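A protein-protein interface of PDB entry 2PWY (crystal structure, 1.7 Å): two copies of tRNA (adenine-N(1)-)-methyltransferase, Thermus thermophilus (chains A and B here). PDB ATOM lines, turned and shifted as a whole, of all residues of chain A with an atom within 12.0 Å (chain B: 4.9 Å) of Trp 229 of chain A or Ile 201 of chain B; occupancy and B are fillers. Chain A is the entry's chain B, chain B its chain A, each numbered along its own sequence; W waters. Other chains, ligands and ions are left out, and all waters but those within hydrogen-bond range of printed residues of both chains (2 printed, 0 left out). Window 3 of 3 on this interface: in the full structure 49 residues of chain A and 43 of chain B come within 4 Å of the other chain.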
ATOM      1  N   GLY A  17       2.296  -5.023 -24.612  1.00  0.00           N
ATOM      2  CA  GLY A  17       2.067  -6.097 -23.640  1.00  0.00           C
ATOM      3  C   GLY A  17       2.164  -7.531 -24.150  1.00  0.00           C
ATOM      4  O   GLY A  17       2.288  -8.463 -23.350  1.00  0.00           O
ATOM      5  N   GLU A  67       2.722 -18.847 -14.826  1.00  0.00           N
ATOM      6  CA  GLU A  67       1.556 -18.182 -15.372  1.00  0.00           C
ATOM      7  C   GLU A  67       1.769 -17.840 -16.857  1.00  0.00           C
ATOM      8  O   GLU A  67       0.934 -18.184 -17.710  1.00  0.00           O
ATOM      9  CB  GLU A  67       1.243 -16.923 -14.558  1.00  0.00           C
ATOM     10  CG  GLU A  67       0.062 -16.116 -15.105  1.00  0.00           C
ATOM     11  CD  GLU A  67      -0.200 -14.823 -14.347  1.00  0.00           C
ATOM     12  OE1 GLU A  67       0.720 -14.311 -13.677  1.00  0.00           O
ATOM     13  OE2 GLU A  67      -1.333 -14.299 -14.445  1.00  0.00           O
ATOM     14  N   GLY A 225     -11.997 -14.674  -9.749  1.00  0.00           N
ATOM     15  CA  GLY A 225     -11.770 -13.515 -10.603  1.00  0.00           C
ATOM     16  C   GLY A 225     -10.488 -12.824 -10.203  1.00  0.00           C
ATOM     17  O   GLY A 225     -10.249 -12.578  -9.013  1.00  0.00           O
ATOM     18  N   TRP A 226      -9.651 -12.527 -11.196  1.00  0.00           N
ATOM     19  CA  TRP A 226      -8.474 -11.689 -10.982  1.00  0.00           C
ATOM     20  C   TRP A 226      -8.699 -10.445 -11.816  1.00  0.00           C
ATOM     21  O   TRP A 226      -8.501 -10.447 -13.039  1.00  0.00           O
ATOM     22  CB  TRP A 226      -7.183 -12.397 -11.409  1.00  0.00           C
ATOM     23  CG  TRP A 226      -6.663 -13.440 -10.450  1.00  0.00           C
ATOM     24  CD1 TRP A 226      -7.315 -13.984  -9.366  1.00  0.00           C
ATOM     25  CD2 TRP A 226      -5.393 -14.090 -10.520  1.00  0.00           C
ATOM     26  NE1 TRP A 226      -6.510 -14.925  -8.757  1.00  0.00           N
ATOM     27  CE2 TRP A 226      -5.327 -15.009  -9.446  1.00  0.00           C
ATOM     28  CE3 TRP A 226      -4.293 -13.984 -11.386  1.00  0.00           C
ATOM     29  CZ2 TRP A 226      -4.199 -15.813  -9.209  1.00  0.00           C
ATOM     30  CZ3 TRP A 226      -3.159 -14.798 -11.146  1.00  0.00           C
ATOM     31  CH2 TRP A 226      -3.131 -15.696 -10.071  1.00  0.00           C
ATOM     32  N   ARG A 227      -9.143  -9.403 -11.130  1.00  0.00           N
ATOM     33  CA  ARG A 227      -9.573  -8.170 -11.767  1.00  0.00           C
ATOM     34  C   ARG A 227      -8.378  -7.245 -11.856  1.00  0.00           C
ATOM     35  O   ARG A 227      -7.939  -6.684 -10.850  1.00  0.00           O
ATOM     36  CB  ARG A 227     -10.690  -7.542 -10.943  1.00  0.00           C
ATOM     37  CG  ARG A 227     -11.323  -6.299 -11.551  1.00  0.00           C
ATOM     38  CD  ARG A 227     -12.510  -5.900 -10.674  1.00  0.00           C
ATOM     39  NE  ARG A 227     -13.107  -4.599 -10.980  1.00  0.00           N
ATOM     40  CZ  ARG A 227     -13.888  -4.359 -12.030  1.00  0.00           C
ATOM     41  NH1 ARG A 227     -14.139  -5.318 -12.917  1.00  0.00           N
ATOM     42  NH2 ARG A 227     -14.397  -3.152 -12.212  1.00  0.00           N
ATOM     43  N   GLU A 228      -7.886  -7.075 -13.080  1.00  0.00           N
ATOM     44  CA  GLU A 228      -6.688  -6.304 -13.350  1.00  0.00           C
ATOM     45  C   GLU A 228      -7.026  -4.830 -13.451  1.00  0.00           C
ATOM     46  O   GLU A 228      -8.064  -4.468 -14.001  1.00  0.00           O
ATOM     47  CB  GLU A 228      -6.029  -6.774 -14.653  1.00  0.00           C
ATOM     48  CG  GLU A 228      -5.756  -8.298 -14.721  1.00  0.00           C
ATOM     49  CD  GLU A 228      -4.492  -8.743 -13.992  1.00  0.00           C
ATOM     50  OE1 GLU A 228      -3.723  -7.887 -13.505  1.00  0.00           O
ATOM     51  OE2 GLU A 228      -4.265  -9.971 -13.908  1.00  0.00           O
ATOM     52  N   TRP A 229      -6.155  -4.004 -12.881  1.00  0.00           N
ATOM     53  CA  TRP A 229      -6.213  -2.561 -13.039  1.00  0.00           C
ATOM     54  C   TRP A 229      -5.141  -2.069 -13.991  1.00  0.00           C
ATOM     55  O   TRP A 229      -4.053  -2.645 -14.059  1.00  0.00           O
ATOM     56  CB  TRP A 229      -5.980  -1.883 -11.692  1.00  0.00           C
ATOM     57  CG  TRP A 229      -7.152  -1.936 -10.772  1.00  0.00           C
ATOM     58  CD1 TRP A 229      -7.795  -3.048 -10.299  1.00  0.00           C
ATOM     59  CD2 TRP A 229      -7.809  -0.809 -10.190  1.00  0.00           C
ATOM     60  NE1 TRP A 229      -8.821  -2.674  -9.455  1.00  0.00           N
ATOM     61  CE2 TRP A 229      -8.848  -1.304  -9.372  1.00  0.00           C
ATOM     62  CE3 TRP A 229      -7.609   0.580 -10.271  1.00  0.00           C
ATOM     63  CZ2 TRP A 229      -9.707  -0.454  -8.657  1.00  0.00           C
ATOM     64  CZ3 TRP A 229      -8.463   1.427  -9.551  1.00  0.00           C
ATOM     65  CH2 TRP A 229      -9.498   0.901  -8.763  1.00  0.00           C
ATOM     66  N   GLU A 230      -5.459  -0.996 -14.709  1.00  0.00           N
ATOM     67  CA  GLU A 230      -4.442  -0.183 -15.368  1.00  0.00           C
ATOM     68  C   GLU A 230      -4.117   1.006 -14.472  1.00  0.00           C
ATOM     69  O   GLU A 230      -5.003   1.806 -14.141  1.00  0.00           O
ATOM     70  CB  GLU A 230      -4.903   0.314 -16.737  1.00  0.00           C
ATOM     71  CG  GLU A 230      -3.916   1.353 -17.305  1.00  0.00           C
ATOM     72  CD  GLU A 230      -3.953   1.494 -18.807  1.00  0.00           C
ATOM     73  OE1 GLU A 230      -5.013   1.226 -19.426  1.00  0.00           O
ATOM     74  OE2 GLU A 230      -2.906   1.902 -19.364  1.00  0.00           O
ATOM     75  N   VAL A 231      -2.850   1.116 -14.076  1.00  0.00           N
ATOM     76  CA  VAL A 231      -2.393   2.259 -13.284  1.00  0.00           C
ATOM     77  C   VAL A 231      -1.174   2.902 -13.947  1.00  0.00           C
ATOM     78  O   VAL A 231      -0.062   2.374 -13.879  1.00  0.00           O
ATOM     79  CB  VAL A 231      -2.060   1.880 -11.812  1.00  0.00           C
ATOM     80  CG1 VAL A 231      -1.598   3.109 -11.035  1.00  0.00           C
ATOM     81  CG2 VAL A 231      -3.276   1.249 -11.111  1.00  0.00           C
ATOM     82  N   ARG A 232      -1.412   4.026 -14.607  1.00  0.00           N
ATOM     83  CA  ARG A 232      -0.342   4.870 -15.119  1.00  0.00           C
ATOM     84  C   ARG A 232      -0.809   6.317 -14.942  1.00  0.00           C
ATOM     85  O   ARG A 232      -1.462   6.866 -15.819  1.00  0.00           O
ATOM     86  CB  ARG A 232      -0.034   4.543 -16.582  1.00  0.00           C
ATOM     87  N   LEU A 233      -0.479   6.904 -13.793  1.00  0.00           N
ATOM     88  CA  LEU A 233      -1.074   8.165 -13.329  1.00  0.00           C
ATOM     89  C   LEU A 233      -0.915   9.294 -14.339  1.00  0.00           C
ATOM     90  O   LEU A 233       0.187   9.515 -14.849  1.00  0.00           O
ATOM     91  CB  LEU A 233      -0.510   8.570 -11.960  1.00  0.00           C
ATOM     92  N   PRO A 234      -2.003  10.045 -14.609  1.00  0.00           N
ATOM     93  CA  PRO A 234      -3.308  10.124 -13.935  1.00  0.00           C
ATOM     94  C   PRO A 234      -4.245   8.914 -14.068  1.00  0.00           C
ATOM     95  O   PRO A 234      -5.165   8.791 -13.258  1.00  0.00           O
ATOM     96  N   VAL A 235      -4.028   8.053 -15.071  1.00  0.00           N
ATOM     97  CA  VAL A 235      -4.917   6.912 -15.349  1.00  0.00           C
ATOM     98  C   VAL A 235      -4.844   5.842 -14.255  1.00  0.00           C
ATOM     99  O   VAL A 235      -3.762   5.407 -13.870  1.00  0.00           O
ATOM    100  CB  VAL A 235      -4.602   6.263 -16.719  1.00  0.00           C
ATOM    101  CG1 VAL A 235      -5.476   5.035 -16.970  1.00  0.00           C
ATOM    102  CG2 VAL A 235      -4.746   7.282 -17.848  1.00  0.00           C
ATOM    103  N   ALA A 236      -6.008   5.417 -13.769  1.00  0.00           N
ATOM    104  CA  ALA A 236      -6.076   4.440 -12.690  1.00  0.00           C
ATOM    105  C   ALA A 236      -7.487   3.874 -12.573  1.00  0.00           C
ATOM    106  O   ALA A 236      -8.362   4.472 -11.942  1.00  0.00           O
ATOM    107  CB  ALA A 236      -5.613   5.064 -11.364  1.00  0.00           C
ATOM    108  N   HIS A 237      -7.707   2.731 -13.217  1.00  0.00           N
ATOM    109  CA  HIS A 237      -9.023   2.079 -13.199  1.00  0.00           C
ATOM    110  C   HIS A 237      -8.914   0.601 -13.524  1.00  0.00           C
ATOM    111  O   HIS A 237      -7.966   0.179 -14.189  1.00  0.00           O
ATOM    112  CB  HIS A 237      -9.964   2.735 -14.217  1.00  0.00           C
ATOM    113  CG  HIS A 237      -9.440   2.728 -15.622  1.00  0.00           C
ATOM    114  ND1 HIS A 237      -9.505   1.616 -16.434  1.00  0.00           N
ATOM    115  CD2 HIS A 237      -8.848   3.698 -16.360  1.00  0.00           C
ATOM    116  CE1 HIS A 237      -8.969   1.899 -17.608  1.00  0.00           C
ATOM    117  NE2 HIS A 237      -8.569   3.157 -17.593  1.00  0.00           N
ATOM    118  N   PRO A 238      -9.906  -0.196 -13.085  1.00  0.00           N
ATOM    119  CA  PRO A 238      -9.921  -1.578 -13.557  1.00  0.00           C
ATOM    120  C   PRO A 238      -9.933  -1.587 -15.079  1.00  0.00           C
ATOM    121  O   PRO A 238     -10.528  -0.701 -15.713  1.00  0.00           O
ATOM    122  CB  PRO A 238     -11.220  -2.152 -12.981  1.00  0.00           C
ATOM    123  CG  PRO A 238     -11.552  -1.257 -11.795  1.00  0.00           C
ATOM    124  CD  PRO A 238     -11.014   0.110 -12.160  1.00  0.00           C
ATOM    125  N   ARG A 239      -9.250  -2.563 -15.662  1.00  0.00           N
ATOM    126  CA  ARG A 239      -9.101  -2.607 -17.110  1.00  0.00           C
ATOM    127  C   ARG A 239     -10.466  -2.686 -17.775  1.00  0.00           C
ATOM    128  O   ARG A 239     -11.360  -3.374 -17.284  1.00  0.00           O
ATOM    129  CB  ARG A 239      -8.202  -3.760 -17.539  1.00  0.00           C
ATOM    130  CG  ARG A 239      -6.751  -3.489 -17.204  1.00  0.00           C
ATOM    131  CD  ARG A 239      -5.808  -4.432 -17.917  1.00  0.00           C
ATOM    132  NE  ARG A 239      -4.444  -4.242 -17.432  1.00  0.00           N
ATOM    133  CZ  ARG A 239      -3.623  -3.279 -17.851  1.00  0.00           C
ATOM    134  NH1 ARG A 239      -4.010  -2.412 -18.782  1.00  0.00           N
ATOM    135  NH2 ARG A 239      -2.399  -3.191 -17.345  1.00  0.00           N
ATOM    136  N   PHE A 240     -10.608  -1.951 -18.877  1.00  0.00           N
ATOM    137  CA  PHE A 240     -11.867  -1.867 -19.602  1.00  0.00           C
ATOM    138  C   PHE A 240     -12.287  -3.247 -20.090  1.00  0.00           C
ATOM    139  O   PHE A 240     -13.480  -3.576 -20.063  1.00  0.00           O
ATOM    140  CB  PHE A 240     -11.762  -0.886 -20.780  1.00  0.00           C
ATOM    141  CG  PHE A 240     -11.546   0.559 -20.373  1.00  0.00           C
ATOM    142  CD1 PHE A 240     -12.372   1.170 -19.426  1.00  0.00           C
ATOM    143  CD2 PHE A 240     -10.534   1.319 -20.969  1.00  0.00           C
ATOM    144  CE1 PHE A 240     -12.184   2.500 -19.055  1.00  0.00           C
ATOM    145  CE2 PHE A 240     -10.336   2.652 -20.612  1.00  0.00           C
ATOM    146  CZ  PHE A 240     -11.168   3.249 -19.652  1.00  0.00           C
ATOM    147  N   GLN A 241     -11.305  -4.044 -20.517  1.00  0.00           N
ATOM    148  CA  GLN A 241     -11.522  -5.418 -20.963  1.00  0.00           C
ATOM    149  C   GLN A 241     -10.894  -6.426 -20.000  1.00  0.00           C
ATOM    150  O   GLN A 241      -9.699  -6.354 -19.695  1.00  0.00           O
ATOM    151  CB  GLN A 241     -10.946  -5.624 -22.366  1.00  0.00           C
ATOM    152  N   GLN A 242     -11.705  -7.370 -19.532  1.00  0.00           N
ATOM    153  CA  GLN A 242     -11.246  -8.426 -18.630  1.00  0.00           C
ATOM    154  C   GLN A 242     -11.722  -9.775 -19.144  1.00  0.00           C
ATOM    155  O   GLN A 242     -12.668  -9.840 -19.935  1.00  0.00           O
ATOM    156  CB  GLN A 242     -11.855  -8.245 -17.238  1.00  0.00           C
ATOM    157  CG  GLN A 242     -11.678  -6.890 -16.604  1.00  0.00           C
ATOM    158  CD  GLN A 242     -10.452  -6.799 -15.714  1.00  0.00           C
ATOM    159  OE1 GLN A 242      -9.779  -7.799 -15.417  1.00  0.00           O
ATOM    160  NE2 GLN A 242     -10.166  -5.589 -15.270  1.00  0.00           N
ATOM    161  N   VAL A 243     -11.089 -10.844 -18.660  1.00  0.00           N
ATOM    162  CA  VAL A 243     -11.666 -12.185 -18.745  1.00  0.00           C
ATOM    163  C   VAL A 243     -12.888 -12.214 -17.825  1.00  0.00           C
ATOM    164  O   VAL A 243     -12.764 -12.013 -16.618  1.00  0.00           O
ATOM    165  CB  VAL A 243     -10.661 -13.282 -18.316  1.00  0.00           C
ATOM    166  CG1 VAL A 243     -11.206 -14.677 -18.642  1.00  0.00           C
ATOM    167  CG2 VAL A 243      -9.304 -13.075 -18.991  1.00  0.00           C
ATOM    168  N   PRO B 199      -4.686  -2.880   1.566  1.00  0.00           N
ATOM    169  CA  PRO B 199      -6.148  -2.735   1.582  1.00  0.00           C
ATOM    170  C   PRO B 199      -6.708  -1.547   0.784  1.00  0.00           C
ATOM    171  O   PRO B 199      -7.791  -1.673   0.183  1.00  0.00           O
ATOM    172  CB  PRO B 199      -6.483  -2.569   3.072  1.00  0.00           C
ATOM    173  CG  PRO B 199      -5.256  -3.015   3.810  1.00  0.00           C
ATOM    174  CD  PRO B 199      -4.098  -2.707   2.909  1.00  0.00           C
ATOM    175  N   ASN B 200      -6.002  -0.420   0.789  1.00  0.00           N
ATOM    176  CA  ASN B 200      -6.543   0.837   0.264  1.00  0.00           C
ATOM    177  C   ASN B 200      -5.940   1.207  -1.079  1.00  0.00           C
ATOM    178  O   ASN B 200      -4.722   1.086  -1.283  1.00  0.00           O
ATOM    179  CB  ASN B 200      -6.299   1.990   1.255  1.00  0.00           C
ATOM    180  CG  ASN B 200      -7.115   1.843   2.522  1.00  0.00           C
ATOM    181  OD1 ASN B 200      -8.319   2.084   2.523  1.00  0.00           O
ATOM    182  ND2 ASN B 200      -6.463   1.446   3.607  1.00  0.00           N
ATOM    183  N   ILE B 201      -6.781   1.688  -1.987  1.00  0.00           N
ATOM    184  CA  ILE B 201      -6.271   2.145  -3.280  1.00  0.00           C
ATOM    185  C   ILE B 201      -5.298   3.330  -3.131  1.00  0.00           C
ATOM    186  O   ILE B 201      -4.402   3.510  -3.957  1.00  0.00           O
ATOM    187  CB  ILE B 201      -7.419   2.472  -4.269  1.00  0.00           C
ATOM    188  CG1 ILE B 201      -6.920   2.415  -5.729  1.00  0.00           C
ATOM    189  CG2 ILE B 201      -8.052   3.828  -3.947  1.00  0.00           C
ATOM    190  CD1 ILE B 201      -6.370   1.041  -6.173  1.00  0.00           C
ATOM    191  N   THR B 202      -5.481   4.131  -2.078  1.00  0.00           N
ATOM    192  CA  THR B 202      -4.583   5.251  -1.790  1.00  0.00           C
ATOM    193  C   THR B 202      -3.163   4.732  -1.475  1.00  0.00           C
ATOM    194  O   THR B 202      -2.167   5.301  -1.922  1.00  0.00           O
ATOM    195  CB  THR B 202      -5.116   6.079  -0.609  1.00  0.00           C
ATOM    196  OG1 THR B 202      -5.598   5.182   0.395  1.00  0.00           O
ATOM    197  CG2 THR B 202      -6.268   6.978  -1.066  1.00  0.00           C
ATOM    198  N   GLN B 203      -3.093   3.623  -0.740  1.00  0.00           N
ATOM    199  CA  GLN B 203      -1.819   2.972  -0.443  1.00  0.00           C
ATOM    200  C   GLN B 203      -1.188   2.429  -1.726  1.00  0.00           C
ATOM    201  O   GLN B 203       0.021   2.560  -1.932  1.00  0.00           O
ATOM    202  CB  GLN B 203      -2.020   1.834   0.552  1.00  0.00           C
ATOM    203  CG  GLN B 203      -2.356   2.288   1.958  1.00  0.00           C
ATOM    204  CD  GLN B 203      -2.747   1.111   2.820  1.00  0.00           C
ATOM    205  OE1 GLN B 203      -3.738   0.438   2.554  1.00  0.00           O
ATOM    206  NE2 GLN B 203      -1.948   0.835   3.845  1.00  0.00           N
ATOM    207  N   VAL B 204      -2.017   1.831  -2.585  1.00  0.00           N
ATOM    208  CA  VAL B 204      -1.564   1.339  -3.888  1.00  0.00           C
ATOM    209  C   VAL B 204      -0.916   2.459  -4.695  1.00  0.00           C
ATOM    210  O   VAL B 204       0.193   2.314  -5.196  1.00  0.00           O
ATOM    211  CB  VAL B 204      -2.720   0.693  -4.702  1.00  0.00           C
ATOM    212  CG1 VAL B 204      -2.286   0.414  -6.169  1.00  0.00           C
ATOM    213  CG2 VAL B 204      -3.213  -0.597  -4.012  1.00  0.00           C
ATOM    214  N   LEU B 205      -1.603   3.591  -4.802  1.00  0.00           N
ATOM    215  CA  LEU B 205      -1.087   4.704  -5.583  1.00  0.00           C
ATOM    216  C   LEU B 205       0.210   5.233  -4.988  1.00  0.00           C
ATOM    217  O   LEU B 205       1.136   5.566  -5.728  1.00  0.00           O
ATOM    218  CB  LEU B 205      -2.146   5.816  -5.711  1.00  0.00           C
ATOM    219  CG  LEU B 205      -3.376   5.421  -6.541  1.00  0.00           C
ATOM    220  CD1 LEU B 205      -4.518   6.412  -6.281  1.00  0.00           C
ATOM    221  CD2 LEU B 205      -3.027   5.346  -8.030  1.00  0.00           C
ATOM    222  N   VAL B 221      -1.616  -4.563 -10.939  1.00  0.00           N
ATOM    223  CA  VAL B 221      -2.421  -4.166  -9.804  1.00  0.00           C
ATOM    224  C   VAL B 221      -3.723  -4.942  -9.960  1.00  0.00           C
ATOM    225  O   VAL B 221      -4.418  -4.802 -10.964  1.00  0.00           O
ATOM    226  CB  VAL B 221      -2.693  -2.659  -9.765  1.00  0.00           C
ATOM    227  CG1 VAL B 221      -3.740  -2.336  -8.656  1.00  0.00           C
ATOM    228  CG2 VAL B 221      -1.395  -1.873  -9.540  1.00  0.00           C
ATOM    229  N   LEU B 222      -4.036  -5.798  -8.996  1.00  0.00           N
ATOM    230  CA  LEU B 222      -5.255  -6.586  -9.140  1.00  0.00           C
ATOM    231  C   LEU B 222      -6.011  -6.829  -7.851  1.00  0.00           C
ATOM    232  O   LEU B 222      -5.467  -6.657  -6.752  1.00  0.00           O
ATOM    233  CB  LEU B 222      -4.977  -7.893  -9.881  1.00  0.00           C
ATOM    234  CG  LEU B 222      -4.040  -8.914  -9.237  1.00  0.00           C
ATOM    235  CD1 LEU B 222      -4.859  -9.798  -8.359  1.00  0.00           C
ATOM    236  CD2 LEU B 222      -3.360  -9.755 -10.309  1.00  0.00           C
ATOM    237  N   GLU B 223      -7.279  -7.192  -8.020  1.00  0.00           N
ATOM    238  CA  GLU B 223      -8.143  -7.624  -6.936  1.00  0.00           C
ATOM    239  C   GLU B 223      -8.540  -9.066  -7.192  1.00  0.00           C
ATOM    240  O   GLU B 223      -9.080  -9.398  -8.263  1.00  0.00           O
ATOM    241  CB  GLU B 223      -9.438  -6.806  -6.905  1.00  0.00           C
ATOM    242  CG  GLU B 223      -9.289  -5.323  -6.823  1.00  0.00           C
ATOM    243  CD  GLU B 223     -10.622  -4.642  -7.010  1.00  0.00           C
ATOM    244  OE1 GLU B 223     -10.733  -3.769  -7.897  1.00  0.00           O
ATOM    245  OE2 GLU B 223     -11.573  -5.016  -6.282  1.00  0.00           O
ATOM    246  N   PHE B 248      -5.769  -5.072  -2.362  1.00  0.00           N
ATOM    247  CA  PHE B 248      -5.188  -5.097  -3.684  1.00  0.00           C
ATOM    248  C   PHE B 248      -3.836  -5.779  -3.635  1.00  0.00           C
ATOM    249  O   PHE B 248      -3.142  -5.693  -2.624  1.00  0.00           O
ATOM    250  CB  PHE B 248      -5.002  -3.664  -4.178  1.00  0.00           C
ATOM    251  CG  PHE B 248      -6.282  -2.902  -4.249  1.00  0.00           C
ATOM    252  CD1 PHE B 248      -7.073  -2.991  -5.382  1.00  0.00           C
ATOM    253  CD2 PHE B 248      -6.716  -2.130  -3.173  1.00  0.00           C
ATOM    254  CE1 PHE B 248      -8.294  -2.312  -5.457  1.00  0.00           C
ATOM    255  CE2 PHE B 248      -7.928  -1.425  -3.246  1.00  0.00           C
ATOM    256  CZ  PHE B 248      -8.714  -1.530  -4.378  1.00  0.00           C
HETATM  257  O   HOH W   1     -12.253  -9.884  -8.503  1.00  0.00           O
HETATM  258  O   HOH W   2      -2.776  -5.129 -13.681  1.00  0.00           O
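The indole nitrogen (NE1) of Trp 229 of chain A lies within hydrogen-bond range of the side-chain carboxylate (OE1) of Glu 223 of chain B (2.7 Å).
The backbone NH (N) of Trp 229 of chain A lies within hydrogen-bond range of the backbone carbonyl oxygen (O) of Val 221 of chain B (2.7 Å).
The backbone carbonyl oxygen of Gly 225 of chain A lies close to the backbone carbonyl oxygen of Glu 223 of chain B (3.5 Å).
The guanidinium group (NE) of Arg 227 of chain A is in salt-bridge range of the side-chain carboxylate (OE1) of Glu 223 of chain B.
O of Glu 228 of chain A lies within hydrogen-bond range of N of Arg 239 of chain A.
NE2 of Gln 242 of chain A lies within hydrogen-bond range of O of Glu 228 of chain A (2.7 Å).
Among the printed residues, merely in contact across the chains: Trp 226 of chain A with Glu 223 of chain B (3.6 Å), Arg 227 of chain A with Val 221 of chain B (3.99 Å), Arg 227 of chain A with Leu 222 of chain B (3.2 Å), Glu 228 of chain A with Val 221 of chain B (3.6 Å), Glu 228 of chain A with Leu 222 of chain B (3.7 Å), Trp 229 of chain A with Ile 201 of chain B (3.99 Å), Trp 229 of chain A with Phe 248 of chain B (3.96 Å) and Val 231 of chain A with Val 221 of chain B (3.97 Å).
Of the printed residues of chain B, Trp 229 of chain A touches Ile 201, Val 221, Glu 223 and Phe 248.
Of the printed residues of chain A, Ile 201 of chain B touches Trp 229 (3.99 Å).
No residue of chain A comes within 4 Å of Val 204 of chain B.
Leu 222 of chain B touches just these residues of chain A: Arg 227 (3.2 Å) and Glu 228 (3.7 Å).
Glu 223 of chain B touches just these residues of chain A: Gly 225 (3.5 Å), Trp 226 (3.6 Å), Arg 227 (2.9 Å) and Trp 229 (2.7 Å).
Of the printed residues of chain B, Gly 225 of chain A touches Glu 223.
Of the printed residues of chain B, Val 231 of chain A touches Val 221 (3.97 Å).
Of the printed residues of chain B, Trp 226 of chain A touches Glu 223 (3.6 Å).
Printed residues of chain B within 4 Å of Glu 228 of chain A: Val 221 and Leu 222.
Glu 67 of chain A touches none of the printed residues of chain B.
Arg 232 of chain A touches none of the printed residues of chain B.
The nearest printed residue of chain A that does not touch Ile 201 of chain B is Val 231 of chain A (5.8 Å).
Of the 21 printed residues of chain A, 6 touch a printed residue of chain B.
Hydrophobic or aromatic side chains of chain A within 4 Å of the printed part of chain B: Trp 229 and Val 231.
Of the 11 printed residues of chain B, 5 touch a printed residue of chain A.
Hydrophobic or aromatic side chains of chain B within 4 Å of the printed part of chain A: Ile 201, Val 221, Leu 222 and Phe 248.
Among the printed residues, 12 pairs touch across the chains.
Among the printed residues, Asp or Glu carboxylates within 4 Å of a Lys or Arg side-chain nitrogen of the other chain: Arg 227 of chain A with Glu 223 of chain B (3.98 Å).
No position is printed for both chains.
Of the 12 pairs that touch across the chains among the printed residues, none has its exchanged pair printed and touching as well.
Water W2 lies within hydrogen-bond range of the backbone carbonyl oxygen (O) of Trp 229 of chain A (2.8 Å), the side-chain carboxylate (OE1) of Glu 228 of chain A (2.9 Å) and the backbone NH (N) of Val 221 of chain B (3.0 Å).
Water W1 lies within hydrogen-bond range of O of Glu 223 of chain B (3.2 Å) and O of Gly 225 of chain A (3.4 Å).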
